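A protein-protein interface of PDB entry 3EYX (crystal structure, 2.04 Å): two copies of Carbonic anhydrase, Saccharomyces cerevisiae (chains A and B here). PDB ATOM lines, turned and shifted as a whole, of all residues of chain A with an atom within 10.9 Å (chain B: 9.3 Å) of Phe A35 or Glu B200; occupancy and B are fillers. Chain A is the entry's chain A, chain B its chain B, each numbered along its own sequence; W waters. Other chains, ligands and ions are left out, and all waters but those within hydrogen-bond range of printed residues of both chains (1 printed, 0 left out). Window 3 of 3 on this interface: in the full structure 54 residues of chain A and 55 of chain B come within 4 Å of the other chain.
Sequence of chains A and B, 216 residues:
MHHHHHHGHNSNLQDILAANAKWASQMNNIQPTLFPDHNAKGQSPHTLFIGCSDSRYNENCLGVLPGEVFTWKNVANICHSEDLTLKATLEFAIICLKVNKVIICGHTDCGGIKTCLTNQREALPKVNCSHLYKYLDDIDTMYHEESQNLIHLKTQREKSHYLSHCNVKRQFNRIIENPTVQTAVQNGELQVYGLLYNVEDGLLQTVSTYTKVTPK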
ATOM      1  N   ASN A  20      -2.487  12.340 -21.089  1.00  0.00           N
ATOM      2  CA  ASN A  20      -3.401  12.885 -22.089  1.00  0.00           C
ATOM      3  C   ASN A  20      -4.004  14.243 -21.704  1.00  0.00           C
ATOM      4  O   ASN A  20      -4.061  15.143 -22.535  1.00  0.00           O
ATOM      5  CB  ASN A  20      -4.508  11.873 -22.411  1.00  0.00           C
ATOM      6  CG  ASN A  20      -5.711  12.523 -23.054  1.00  0.00           C
ATOM      7  OD1 ASN A  20      -6.740  12.684 -22.407  1.00  0.00           O
ATOM      8  ND2 ASN A  20      -5.584  12.916 -24.328  1.00  0.00           N
ATOM      9  N   ALA A  21      -4.443  14.382 -20.451  1.00  0.00           N
ATOM     10  CA  ALA A  21      -5.019  15.645 -19.948  1.00  0.00           C
ATOM     11  C   ALA A  21      -4.029  16.822 -20.015  1.00  0.00           C
ATOM     12  O   ALA A  21      -4.410  17.945 -20.359  1.00  0.00           O
ATOM     13  CB  ALA A  21      -5.552  15.474 -18.521  1.00  0.00           C
ATOM     14  N   LYS A  22      -2.773  16.545 -19.676  1.00  0.00           N
ATOM     15  CA  LYS A  22      -1.683  17.509 -19.780  1.00  0.00           C
ATOM     16  C   LYS A  22      -1.496  17.909 -21.235  1.00  0.00           C
ATOM     17  O   LYS A  22      -1.499  19.099 -21.565  1.00  0.00           O
ATOM     18  CB  LYS A  22      -0.394  16.895 -19.225  1.00  0.00           C
ATOM     19  CG  LYS A  22       0.818  17.806 -19.266  1.00  0.00           C
ATOM     20  CD  LYS A  22       2.107  17.014 -19.059  1.00  0.00           C
ATOM     21  CE  LYS A  22       3.275  17.915 -18.629  1.00  0.00           C
ATOM     22  NZ  LYS A  22       3.386  19.139 -19.465  1.00  0.00           N
ATOM     23  N   TRP A  23      -1.362  16.901 -22.097  1.00  0.00           N
ATOM     24  CA  TRP A  23      -1.179  17.099 -23.535  1.00  0.00           C
ATOM     25  C   TRP A  23      -2.320  17.904 -24.158  1.00  0.00           C
ATOM     26  O   TRP A  23      -2.083  18.781 -24.992  1.00  0.00           O
ATOM     27  CB  TRP A  23      -1.023  15.743 -24.242  1.00  0.00           C
ATOM     28  CG  TRP A  23      -1.072  15.838 -25.745  1.00  0.00           C
ATOM     29  CD1 TRP A  23      -0.014  16.011 -26.592  1.00  0.00           C
ATOM     30  CD2 TRP A  23      -2.241  15.763 -26.575  1.00  0.00           C
ATOM     31  NE1 TRP A  23      -0.452  16.052 -27.893  1.00  0.00           N
ATOM     32  CE2 TRP A  23      -1.815  15.905 -27.910  1.00  0.00           C
ATOM     33  CE3 TRP A  23      -3.608  15.585 -26.317  1.00  0.00           C
ATOM     34  CZ2 TRP A  23      -2.708  15.877 -28.987  1.00  0.00           C
ATOM     35  CZ3 TRP A  23      -4.497  15.575 -27.386  1.00  0.00           C
ATOM     36  CH2 TRP A  23      -4.044  15.717 -28.702  1.00  0.00           C
ATOM     37  N   ALA A  24      -3.552  17.587 -23.757  1.00  0.00           N
ATOM     38  CA  ALA A  24      -4.748  18.243 -24.287  1.00  0.00           C
ATOM     39  C   ALA A  24      -4.887  19.702 -23.856  1.00  0.00           C
ATOM     40  O   ALA A  24      -5.300  20.534 -24.661  1.00  0.00           O
ATOM     41  CB  ALA A  24      -6.004  17.460 -23.912  1.00  0.00           C
ATOM     42  N   SER A  25      -4.561  20.003 -22.592  1.00  0.00           N
ATOM     43  CA  SER A  25      -4.620  21.384 -22.095  1.00  0.00           C
ATOM     44  C   SER A  25      -3.625  22.256 -22.847  1.00  0.00           C
ATOM     45  O   SER A  25      -3.941  23.388 -23.225  1.00  0.00           O
ATOM     46  CB  SER A  25      -4.372  21.468 -20.581  1.00  0.00           C
ATOM     47  OG  SER A  25      -3.113  20.921 -20.225  1.00  0.00           O
ATOM     48  N   GLN A  26      -2.430  21.716 -23.082  1.00  0.00           N
ATOM     49  CA  GLN A  26      -1.417  22.409 -23.869  1.00  0.00           C
ATOM     50  C   GLN A  26      -1.850  22.574 -25.320  1.00  0.00           C
ATOM     51  O   GLN A  26      -1.714  23.658 -25.906  1.00  0.00           O
ATOM     52  CB  GLN A  26      -0.086  21.673 -23.775  1.00  0.00           C
ATOM     53  CG  GLN A  26       0.646  21.956 -22.467  1.00  0.00           C
ATOM     54  CD  GLN A  26       1.436  20.772 -21.953  1.00  0.00           C
ATOM     55  OE1 GLN A  26       1.552  20.581 -20.739  1.00  0.00           O
ATOM     56  NE2 GLN A  26       1.992  19.972 -22.867  1.00  0.00           N
ATOM     57  N   MET A  27      -2.404  21.502 -25.881  1.00  0.00           N
ATOM     58  CA  MET A  27      -2.854  21.504 -27.268  1.00  0.00           C
ATOM     59  C   MET A  27      -3.995  22.501 -27.503  1.00  0.00           C
ATOM     60  O   MET A  27      -4.032  23.154 -28.546  1.00  0.00           O
ATOM     61  CB  MET A  27      -3.244  20.087 -27.708  1.00  0.00           C
ATOM     62  CG  MET A  27      -2.901  19.767 -29.150  1.00  0.00           C
ATOM     63  SD  MET A  27      -1.168  20.059 -29.619  1.00  0.00           S
ATOM     64  CE  MET A  27      -1.295  19.766 -31.377  1.00  0.00           C
ATOM     65  N   ASN A  28      -4.906  22.629 -26.537  1.00  0.00           N
ATOM     66  CA  ASN A  28      -5.999  23.611 -26.630  1.00  0.00           C
ATOM     67  C   ASN A  28      -5.457  25.029 -26.776  1.00  0.00           C
ATOM     68  O   ASN A  28      -5.971  25.816 -27.574  1.00  0.00           O
ATOM     69  CB  ASN A  28      -6.933  23.551 -25.412  1.00  0.00           C
ATOM     70  CG  ASN A  28      -7.763  22.265 -25.347  1.00  0.00           C
ATOM     71  OD1 ASN A  28      -8.037  21.615 -26.356  1.00  0.00           O
ATOM     72  ND2 ASN A  28      -8.168  21.902 -24.141  1.00  0.00           N
ATOM     73  N   ASN A  29      -4.416  25.332 -25.996  1.00  0.00           N
ATOM     74  CA  ASN A  29      -3.732  26.627 -26.012  1.00  0.00           C
ATOM     75  C   ASN A  29      -2.971  26.894 -27.312  1.00  0.00           C
ATOM     76  O   ASN A  29      -3.078  27.980 -27.887  1.00  0.00           O
ATOM     77  CB  ASN A  29      -2.754  26.721 -24.832  1.00  0.00           C
ATOM     78  CG  ASN A  29      -3.446  26.912 -23.495  1.00  0.00           C
ATOM     79  OD1 ASN A  29      -4.593  27.347 -23.423  1.00  0.00           O
ATOM     80  ND2 ASN A  29      -2.736  26.594 -22.420  1.00  0.00           N
ATOM     81  N   ILE A  30      -2.211  25.897 -27.770  1.00  0.00           N
ATOM     82  CA  ILE A  30      -1.337  26.048 -28.938  1.00  0.00           C
ATOM     83  C   ILE A  30      -2.111  26.094 -30.256  1.00  0.00           C
ATOM     84  O   ILE A  30      -1.821  26.924 -31.121  1.00  0.00           O
ATOM     85  CB  ILE A  30      -0.273  24.926 -29.003  1.00  0.00           C
ATOM     86  CG1 ILE A  30       0.645  24.986 -27.777  1.00  0.00           C
ATOM     87  CG2 ILE A  30       0.534  25.025 -30.299  1.00  0.00           C
ATOM     88  CD1 ILE A  30       1.297  23.651 -27.421  1.00  0.00           C
ATOM     89  N   GLN A  31      -3.088  25.199 -30.403  1.00  0.00           N
ATOM     90  CA  GLN A  31      -3.834  25.063 -31.653  1.00  0.00           C
ATOM     91  C   GLN A  31      -5.346  25.110 -31.397  1.00  0.00           C
ATOM     92  O   GLN A  31      -6.037  24.087 -31.496  1.00  0.00           O
ATOM     93  CB  GLN A  31      -3.432  23.765 -32.355  1.00  0.00           C
ATOM     94  CG  GLN A  31      -3.676  23.728 -33.864  1.00  0.00           C
ATOM     95  CD  GLN A  31      -3.223  22.416 -34.485  1.00  0.00           C
ATOM     96  OE1 GLN A  31      -2.325  21.754 -33.963  1.00  0.00           O
ATOM     97  NE2 GLN A  31      -3.843  22.031 -35.597  1.00  0.00           N
ATOM     98  N   PRO A  32      -5.876  26.308 -31.094  1.00  0.00           N
ATOM     99  CA  PRO A  32      -7.285  26.370 -30.704  1.00  0.00           C
ATOM    100  C   PRO A  32      -8.239  26.028 -31.859  1.00  0.00           C
ATOM    101  O   PRO A  32      -9.359  25.581 -31.611  1.00  0.00           O
ATOM    102  CB  PRO A  32      -7.458  27.821 -30.246  1.00  0.00           C
ATOM    103  CG  PRO A  32      -6.410  28.581 -30.991  1.00  0.00           C
ATOM    104  CD  PRO A  32      -5.247  27.642 -31.139  1.00  0.00           C
ATOM    105  N   THR A  33      -7.779  26.218 -33.099  1.00  0.00           N
ATOM    106  CA  THR A  33      -8.579  25.941 -34.302  1.00  0.00           C
ATOM    107  C   THR A  33      -8.731  24.442 -34.581  1.00  0.00           C
ATOM    108  O   THR A  33      -9.585  24.041 -35.373  1.00  0.00           O
ATOM    109  CB  THR A  33      -8.007  26.636 -35.580  1.00  0.00           C
ATOM    110  OG1 THR A  33      -6.731  26.072 -35.920  1.00  0.00           O
ATOM    111  CG2 THR A  33      -7.876  28.151 -35.391  1.00  0.00           C
ATOM    112  N   LEU A  34      -7.891  23.626 -33.942  1.00  0.00           N
ATOM    113  CA  LEU A  34      -7.952  22.166 -34.086  1.00  0.00           C
ATOM    114  C   LEU A  34      -9.208  21.604 -33.422  1.00  0.00           C
ATOM    115  O   LEU A  34      -9.802  20.634 -33.900  1.00  0.00           O
ATOM    116  CB  LEU A  34      -6.689  21.513 -33.497  1.00  0.00           C
ATOM    117  CG  LEU A  34      -6.584  19.989 -33.317  1.00  0.00           C
ATOM    118  CD1 LEU A  34      -6.733  19.240 -34.634  1.00  0.00           C
ATOM    119  CD2 LEU A  34      -5.269  19.619 -32.639  1.00  0.00           C
ATOM    120  N   PHE A  35      -9.610  22.245 -32.332  1.00  0.00           N
ATOM    121  CA  PHE A  35     -10.691  21.767 -31.490  1.00  0.00           C
ATOM    122  C   PHE A  35     -11.970  22.570 -31.742  1.00  0.00           C
ATOM    123  O   PHE A  35     -12.389  23.380 -30.909  1.00  0.00           O
ATOM    124  CB  PHE A  35     -10.264  21.836 -30.017  1.00  0.00           C
ATOM    125  CG  PHE A  35      -9.007  21.066 -29.711  1.00  0.00           C
ATOM    126  CD1 PHE A  35      -9.060  19.706 -29.423  1.00  0.00           C
ATOM    127  CD2 PHE A  35      -7.762  21.704 -29.704  1.00  0.00           C
ATOM    128  CE1 PHE A  35      -7.892  18.989 -29.140  1.00  0.00           C
ATOM    129  CE2 PHE A  35      -6.583  20.988 -29.413  1.00  0.00           C
ATOM    130  CZ  PHE A  35      -6.653  19.633 -29.132  1.00  0.00           C
ATOM    131  N   LEU A  65       0.726  20.246 -39.231  1.00  0.00           N
ATOM    132  CA  LEU A  65       0.007  20.271 -37.950  1.00  0.00           C
ATOM    133  C   LEU A  65      -1.103  19.228 -37.974  1.00  0.00           C
ATOM    134  O   LEU A  65      -1.440  18.734 -39.048  1.00  0.00           O
ATOM    135  CB  LEU A  65      -0.572  21.662 -37.682  1.00  0.00           C
ATOM    136  CG  LEU A  65       0.180  22.546 -36.680  1.00  0.00           C
ATOM    137  CD1 LEU A  65       1.610  22.764 -37.111  1.00  0.00           C
ATOM    138  CD2 LEU A  65      -0.533  23.871 -36.513  1.00  0.00           C
ATOM    139  N   PRO A  66      -1.670  18.880 -36.797  1.00  0.00           N
ATOM    140  CA  PRO A  66      -2.806  17.960 -36.794  1.00  0.00           C
ATOM    141  C   PRO A  66      -3.964  18.485 -37.628  1.00  0.00           C
ATOM    142  O   PRO A  66      -4.155  19.709 -37.738  1.00  0.00           O
ATOM    143  CB  PRO A  66      -3.211  17.902 -35.314  1.00  0.00           C
ATOM    144  CG  PRO A  66      -1.970  18.239 -34.583  1.00  0.00           C
ATOM    145  CD  PRO A  66      -1.299  19.277 -35.426  1.00  0.00           C
ATOM    146  N   GLY A  67      -4.720  17.558 -38.212  1.00  0.00           N
ATOM    147  CA  GLY A  67      -5.842  17.907 -39.058  1.00  0.00           C
ATOM    148  C   GLY A  67      -5.469  17.990 -40.523  1.00  0.00           C
ATOM    149  O   GLY A  67      -6.347  18.051 -41.367  1.00  0.00           O
ATOM    150  N   ARG B  56      -7.254  14.234 -37.140  1.00  0.00           N
ATOM    151  CA  ARG B  56      -7.278  15.113 -35.972  1.00  0.00           C
ATOM    152  C   ARG B  56      -6.601  14.523 -34.732  1.00  0.00           C
ATOM    153  O   ARG B  56      -6.313  15.251 -33.796  1.00  0.00           O
ATOM    154  CB  ARG B  56      -8.710  15.558 -35.658  1.00  0.00           C
ATOM    155  CG  ARG B  56      -9.299  16.505 -36.702  1.00  0.00           C
ATOM    156  CD  ARG B  56     -10.811  16.653 -36.528  1.00  0.00           C
ATOM    157  NE  ARG B  56     -11.517  15.391 -36.765  1.00  0.00           N
ATOM    158  CZ  ARG B  56     -12.839  15.230 -36.703  1.00  0.00           C
ATOM    159  NH1 ARG B  56     -13.649  16.252 -36.415  1.00  0.00           N
ATOM    160  NH2 ARG B  56     -13.359  14.032 -36.942  1.00  0.00           N
ATOM    161  N   TYR B  57      -6.348  13.215 -34.735  1.00  0.00           N
ATOM    162  CA  TYR B  57      -5.650  12.556 -33.625  1.00  0.00           C
ATOM    163  C   TYR B  57      -4.785  11.405 -34.112  1.00  0.00           C
ATOM    164  O   TYR B  57      -4.938  10.919 -35.238  1.00  0.00           O
ATOM    165  CB  TYR B  57      -6.629  12.097 -32.513  1.00  0.00           C
ATOM    166  CG  TYR B  57      -7.394  10.785 -32.761  1.00  0.00           C
ATOM    167  CD1 TYR B  57      -7.348   9.750 -31.830  1.00  0.00           C
ATOM    168  CD2 TYR B  57      -8.176  10.599 -33.910  1.00  0.00           C
ATOM    169  CE1 TYR B  57      -8.045   8.555 -32.034  1.00  0.00           C
ATOM    170  CE2 TYR B  57      -8.880   9.400 -34.128  1.00  0.00           C
ATOM    171  CZ  TYR B  57      -8.808   8.387 -33.190  1.00  0.00           C
ATOM    172  OH  TYR B  57      -9.498   7.203 -33.386  1.00  0.00           O
ATOM    173  N   CYS B  61      -1.779  11.740 -28.806  1.00  0.00           N
ATOM    174  CA  CYS B  61      -2.796  12.103 -27.793  1.00  0.00           C
ATOM    175  C   CYS B  61      -2.604  11.416 -26.422  1.00  0.00           C
ATOM    176  O   CYS B  61      -3.127  11.895 -25.401  1.00  0.00           O
ATOM    177  CB  CYS B  61      -4.219  11.856 -28.312  1.00  0.00           C
ATOM    178  SG  CYS B  61      -4.730  10.149 -28.279  1.00  0.00           S
ATOM    179  N   HIS B 107     -12.993   7.691 -31.707  1.00  0.00           N
ATOM    180  CA  HIS B 107     -13.107   9.121 -31.502  1.00  0.00           C
ATOM    181  C   HIS B 107     -14.487   9.601 -31.878  1.00  0.00           C
ATOM    182  O   HIS B 107     -15.209   8.945 -32.641  1.00  0.00           O
ATOM    183  CB  HIS B 107     -12.060   9.883 -32.321  1.00  0.00           C
ATOM    184  CG  HIS B 107     -12.320   9.853 -33.789  1.00  0.00           C
ATOM    185  ND1 HIS B 107     -12.907  10.903 -34.464  1.00  0.00           N
ATOM    186  CD2 HIS B 107     -12.105   8.885 -34.708  1.00  0.00           C
ATOM    187  CE1 HIS B 107     -13.016  10.592 -35.743  1.00  0.00           C
ATOM    188  NE2 HIS B 107     -12.544   9.368 -35.914  1.00  0.00           N
ATOM    189  N   THR B 108     -14.846  10.767 -31.349  1.00  0.00           N
ATOM    190  CA  THR B 108     -16.137  11.358 -31.662  1.00  0.00           C
ATOM    191  C   THR B 108     -16.036  12.041 -33.021  1.00  0.00           C
ATOM    192  O   THR B 108     -14.935  12.383 -33.457  1.00  0.00           O
ATOM    193  CB  THR B 108     -16.599  12.323 -30.556  1.00  0.00           C
ATOM    194  OG1 THR B 108     -15.613  13.340 -30.355  1.00  0.00           O
ATOM    195  CG2 THR B 108     -16.834  11.567 -29.236  1.00  0.00           C
ATOM    196  N   ASP B 109     -17.186  12.205 -33.689  1.00  0.00           N
ATOM    197  CA  ASP B 109     -17.267  12.815 -35.024  1.00  0.00           C
ATOM    198  C   ASP B 109     -16.488  11.985 -36.060  1.00  0.00           C
ATOM    199  O   ASP B 109     -15.677  12.518 -36.831  1.00  0.00           O
ATOM    200  CB  ASP B 109     -16.805  14.290 -34.983  1.00  0.00           C
ATOM    201  CG  ASP B 109     -17.209  15.079 -36.224  1.00  0.00           C
ATOM    202  OD1 ASP B 109     -18.362  14.975 -36.676  1.00  0.00           O
ATOM    203  OD2 ASP B 109     -16.365  15.812 -36.754  1.00  0.00           O
ATOM    204  N   ARG B 157     -25.727  14.859 -33.238  1.00  0.00           N
ATOM    205  CA  ARG B 157     -24.595  14.942 -32.313  1.00  0.00           C
ATOM    206  C   ARG B 157     -24.631  13.853 -31.230  1.00  0.00           C
ATOM    207  O   ARG B 157     -23.615  13.206 -30.967  1.00  0.00           O
ATOM    208  CB  ARG B 157     -24.542  16.345 -31.680  1.00  0.00           C
ATOM    209  CG  ARG B 157     -23.605  16.503 -30.500  1.00  0.00           C
ATOM    210  CD  ARG B 157     -23.605  17.944 -30.016  1.00  0.00           C
ATOM    211  NE  ARG B 157     -22.659  18.143 -28.918  1.00  0.00           N
ATOM    212  CZ  ARG B 157     -21.371  18.441 -29.088  1.00  0.00           C
ATOM    213  NH1 ARG B 157     -20.865  18.581 -30.313  1.00  0.00           N
ATOM    214  NH2 ARG B 157     -20.589  18.606 -28.029  1.00  0.00           N
ATOM    215  N   HIS B 161     -22.218  10.518 -31.066  1.00  0.00           N
ATOM    216  CA  HIS B 161     -21.497  10.203 -29.827  1.00  0.00           C
ATOM    217  C   HIS B 161     -21.755   8.760 -29.355  1.00  0.00           C
ATOM    218  O   HIS B 161     -20.813   8.004 -29.049  1.00  0.00           O
ATOM    219  CB  HIS B 161     -21.844  11.201 -28.715  1.00  0.00           C
ATOM    220  CG  HIS B 161     -21.014  11.023 -27.483  1.00  0.00           C
ATOM    221  ND1 HIS B 161     -19.805  11.662 -27.302  1.00  0.00           N
ATOM    222  CD2 HIS B 161     -21.198  10.249 -26.387  1.00  0.00           C
ATOM    223  CE1 HIS B 161     -19.285  11.298 -26.142  1.00  0.00           C
ATOM    224  NE2 HIS B 161     -20.114  10.445 -25.566  1.00  0.00           N
ATOM    225  N   LEU B 196     -12.099   6.488 -25.893  1.00  0.00           N
ATOM    226  CA  LEU B 196     -12.783   7.335 -26.851  1.00  0.00           C
ATOM    227  C   LEU B 196     -12.210   8.736 -26.774  1.00  0.00           C
ATOM    228  O   LEU B 196     -12.294   9.395 -25.740  1.00  0.00           O
ATOM    229  CB  LEU B 196     -14.299   7.338 -26.617  1.00  0.00           C
ATOM    230  CG  LEU B 196     -15.129   8.293 -27.494  1.00  0.00           C
ATOM    231  CD1 LEU B 196     -15.203   7.777 -28.918  1.00  0.00           C
ATOM    232  CD2 LEU B 196     -16.523   8.490 -26.928  1.00  0.00           C
ATOM    233  N   TYR B 197     -11.619   9.168 -27.886  1.00  0.00           N
ATOM    234  CA  TYR B 197     -11.022  10.490 -28.002  1.00  0.00           C
ATOM    235  C   TYR B 197     -12.078  11.523 -28.399  1.00  0.00           C
ATOM    236  O   TYR B 197     -12.747  11.385 -29.432  1.00  0.00           O
ATOM    237  CB  TYR B 197      -9.887  10.473 -29.034  1.00  0.00           C
ATOM    238  CG  TYR B 197      -9.233  11.825 -29.262  1.00  0.00           C
ATOM    239  CD1 TYR B 197      -8.197  12.266 -28.447  1.00  0.00           C
ATOM    240  CD2 TYR B 197      -9.656  12.657 -30.293  1.00  0.00           C
ATOM    241  CE1 TYR B 197      -7.595  13.502 -28.655  1.00  0.00           C
ATOM    242  CE2 TYR B 197      -9.060  13.894 -30.517  1.00  0.00           C
ATOM    243  CZ  TYR B 197      -8.033  14.310 -29.687  1.00  0.00           C
ATOM    244  OH  TYR B 197      -7.453  15.530 -29.897  1.00  0.00           O
ATOM    245  N   ASN B 198     -12.225  12.563 -27.580  1.00  0.00           N
ATOM    246  CA  ASN B 198     -13.180  13.630 -27.889  1.00  0.00           C
ATOM    247  C   ASN B 198     -12.446  14.693 -28.699  1.00  0.00           C
ATOM    248  O   ASN B 198     -11.534  15.341 -28.181  1.00  0.00           O
ATOM    249  CB  ASN B 198     -13.769  14.192 -26.584  1.00  0.00           C
ATOM    250  CG  ASN B 198     -14.882  15.205 -26.811  1.00  0.00           C
ATOM    251  OD1 ASN B 198     -14.989  15.808 -27.875  1.00  0.00           O
ATOM    252  ND2 ASN B 198     -15.717  15.405 -25.786  1.00  0.00           N
ATOM    253  N   VAL B 199     -12.817  14.840 -29.968  1.00  0.00           N
ATOM    254  CA  VAL B 199     -12.158  15.795 -30.886  1.00  0.00           C
ATOM    255  C   VAL B 199     -12.400  17.268 -30.505  1.00  0.00           C
ATOM    256  O   VAL B 199     -11.662  18.160 -30.928  1.00  0.00           O
ATOM    257  CB  VAL B 199     -12.581  15.598 -32.375  1.00  0.00           C
ATOM    258  CG1 VAL B 199     -12.158  14.220 -32.900  1.00  0.00           C
ATOM    259  CG2 VAL B 199     -14.087  15.839 -32.556  1.00  0.00           C
ATOM    260  N   GLU B 200     -13.436  17.508 -29.710  1.00  0.00           N
ATOM    261  CA  GLU B 200     -13.745  18.865 -29.258  1.00  0.00           C
ATOM    262  C   GLU B 200     -12.813  19.394 -28.157  1.00  0.00           C
ATOM    263  O   GLU B 200     -12.655  20.609 -28.018  1.00  0.00           O
ATOM    264  CB  GLU B 200     -15.208  18.952 -28.840  1.00  0.00           C
ATOM    265  CG  GLU B 200     -16.145  18.936 -30.035  1.00  0.00           C
ATOM    266  CD  GLU B 200     -17.586  19.252 -29.677  1.00  0.00           C
ATOM    267  OE1 GLU B 200     -17.920  19.300 -28.474  1.00  0.00           O
ATOM    268  OE2 GLU B 200     -18.386  19.440 -30.614  1.00  0.00           O
ATOM    269  N   ASP B 201     -12.184  18.499 -27.390  1.00  0.00           N
ATOM    270  CA  ASP B 201     -11.331  18.922 -26.266  1.00  0.00           C
ATOM    271  C   ASP B 201     -10.008  18.149 -26.089  1.00  0.00           C
ATOM    272  O   ASP B 201      -9.223  18.438 -25.171  1.00  0.00           O
ATOM    273  CB  ASP B 201     -12.136  18.971 -24.942  1.00  0.00           C
ATOM    274  CG  ASP B 201     -12.647  17.599 -24.479  1.00  0.00           C
ATOM    275  OD1 ASP B 201     -12.210  16.549 -24.998  1.00  0.00           O
ATOM    276  OD2 ASP B 201     -13.483  17.581 -23.556  1.00  0.00           O
ATOM    277  N   GLY B 202      -9.775  17.159 -26.950  1.00  0.00           N
ATOM    278  CA  GLY B 202      -8.548  16.360 -26.899  1.00  0.00           C
ATOM    279  C   GLY B 202      -8.462  15.355 -25.765  1.00  0.00           C
ATOM    280  O   GLY B 202      -7.408  14.737 -25.567  1.00  0.00           O
ATOM    281  N   LEU B 203      -9.567  15.159 -25.042  1.00  0.00           N
ATOM    282  CA  LEU B 203      -9.583  14.277 -23.874  1.00  0.00           C
ATOM    283  C   LEU B 203     -10.071  12.850 -24.158  1.00  0.00           C
ATOM    284  O   LEU B 203     -11.058  12.641 -24.880  1.00  0.00           O
ATOM    285  CB  LEU B 203     -10.406  14.886 -22.728  1.00  0.00           C
ATOM    286  CG  LEU B 203      -9.912  16.162 -22.026  1.00  0.00           C
ATOM    287  CD1 LEU B 203     -10.908  16.621 -20.962  1.00  0.00           C
ATOM    288  CD2 LEU B 203      -8.537  15.946 -21.401  1.00  0.00           C
ATOM    289  N   LEU B 204      -9.385  11.892 -23.541  1.00  0.00           N
ATOM    290  CA  LEU B 204      -9.729  10.460 -23.607  1.00  0.00           C
ATOM    291  C   LEU B 204     -10.722  10.040 -22.536  1.00  0.00           C
ATOM    292  O   LEU B 204     -10.519  10.259 -21.332  1.00  0.00           O
ATOM    293  CB  LEU B 204      -8.468   9.583 -23.497  1.00  0.00           C
ATOM    294  CG  LEU B 204      -7.446   9.734 -24.630  1.00  0.00           C
ATOM    295  CD1 LEU B 204      -6.112   9.043 -24.302  1.00  0.00           C
ATOM    296  CD2 LEU B 204      -8.019   9.218 -25.952  1.00  0.00           C
HETATM  297  O   HOH W   1      -7.956  12.282 -20.093  1.00  0.00           O
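Among the printed residues, pairs that only touch across the chains: Asn A20 with Leu B203 (3.6 Å), Ala A21 with Leu B203 (3.8 Å), Trp A23 with Cys B61 (3.8 Å), Trp A23 with Tyr B197 (3.6 Å), Trp A23 with Gly B202 (3.5 Å), Ala A24 with Asp B201 (3.6 Å), Ala A24 with Gly B202 (3.5 Å), Ala A24 with Leu B203 (3.9 Å), Asn A28 with Asp B201 (3.6 Å), Phe A35 with Tyr B197 (3.6 Å), Phe A35 with Val B199 (3.4 Å), Phe A35 with Glu B200 (3.3 Å), Phe A35 with Asp B201 (3.8 Å) and Phe A35 with Gly B202 (3.4 Å).
Of the printed residues of chain B, Trp A23 touches Cys B61 (3.8 Å), Tyr B197 (3.6 Å) and Gly B202 (3.5 Å).
Of the printed residues of chain B, Asn A28 touches Asp B201 (3.6 Å).
No residue of chain B comes within 4 Å of Leu A34.
Of the printed residues of chain A, Cys B61 touches Asn A20 (2.9 Å) and Trp A23 (3.8 Å).
Printed residues of chain A within 4 Å of Tyr B197: Trp A23 (3.6 Å) and Phe A35 (3.6 Å).
Val B199 touches just one residue of chain A: Phe A35 (3.4 Å).
Glu B200 touches just one residue of chain A: Phe A35 (3.3 Å).
Asp B201 touches three residues of chain A.
Of chain A, only Asn A20, Trp A23, Ala A24 and Phe A35 come within 4 Å of Gly B202.
Of the printed residues of chain A, Leu B204 touches Asn A20 (3.0 Å).
The nearest residue of chain B that does not touch Phe A35 is Asn B198 (5.2 Å).
The nearest residue of chain A that does not touch Glu B200 is Asn A28 (5.0 Å).
The side-chain amide nitrogen (ND2) of Asn A20 lies within hydrogen-bond range of the backbone carbonyl oxygen (O) of Gly B202, at 2.9 Å.
N of Leu B204 sits at hydrogen-bond distance from OD1 of Asn A20 (3.0 Å).
The side-chain amide nitrogen of Asn A20 is in hydrogen-bond range of the backbone carbonyl oxygen of Cys B61 (2.9 Å).
Hydrophobic or aromatic side chains of chain A within 4 Å of the printed part of chain B: Trp A23, Ala A24 and Phe A35.
Of the 17 printed residues of chain B, 8 touch a printed residue of chain A.
Among the printed residues, 17 pairs touch across the chains.
Among the printed residues, no Asp or Glu carboxylate lies within 4 Å of a Lys or Arg side-chain nitrogen of the other chain.
No position is printed for both chains.
Of the 17 pairs that touch across the chains among the printed residues, none has its exchanged pair printed and touching as well.
The backbone NH (N) of Leu B203 is in hydrogen-bond range of the side-chain carboxylate (OD1) of Asp B201 (3.0 Å).
The side-chain hydroxyl (OG1) of Thr B108 lies within hydrogen-bond range of the backbone NH (N) of Val B199.
The side-chain amide nitrogen of Asn A28 sits close to the backbone carbonyl oxygen of Ala A24, at 3.2 Å.
The side-chain carboxylate (OE2) of Glu B200 is in salt-bridge range of the guanidinium group (NH1) of Arg B157 (2.6 Å).
N of Asn B198 is in hydrogen-bond range of O of Leu B203 (2.9 Å).
The backbone NH of Thr B108 lies within hydrogen-bond range of the backbone carbonyl oxygen of Tyr B197.
Water W1 bridges the side-chain amide oxygen (OD1) of Asn A20 (2.6 Å) and the backbone carbonyl oxygen (O) of Leu B204 (3.5 Å).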
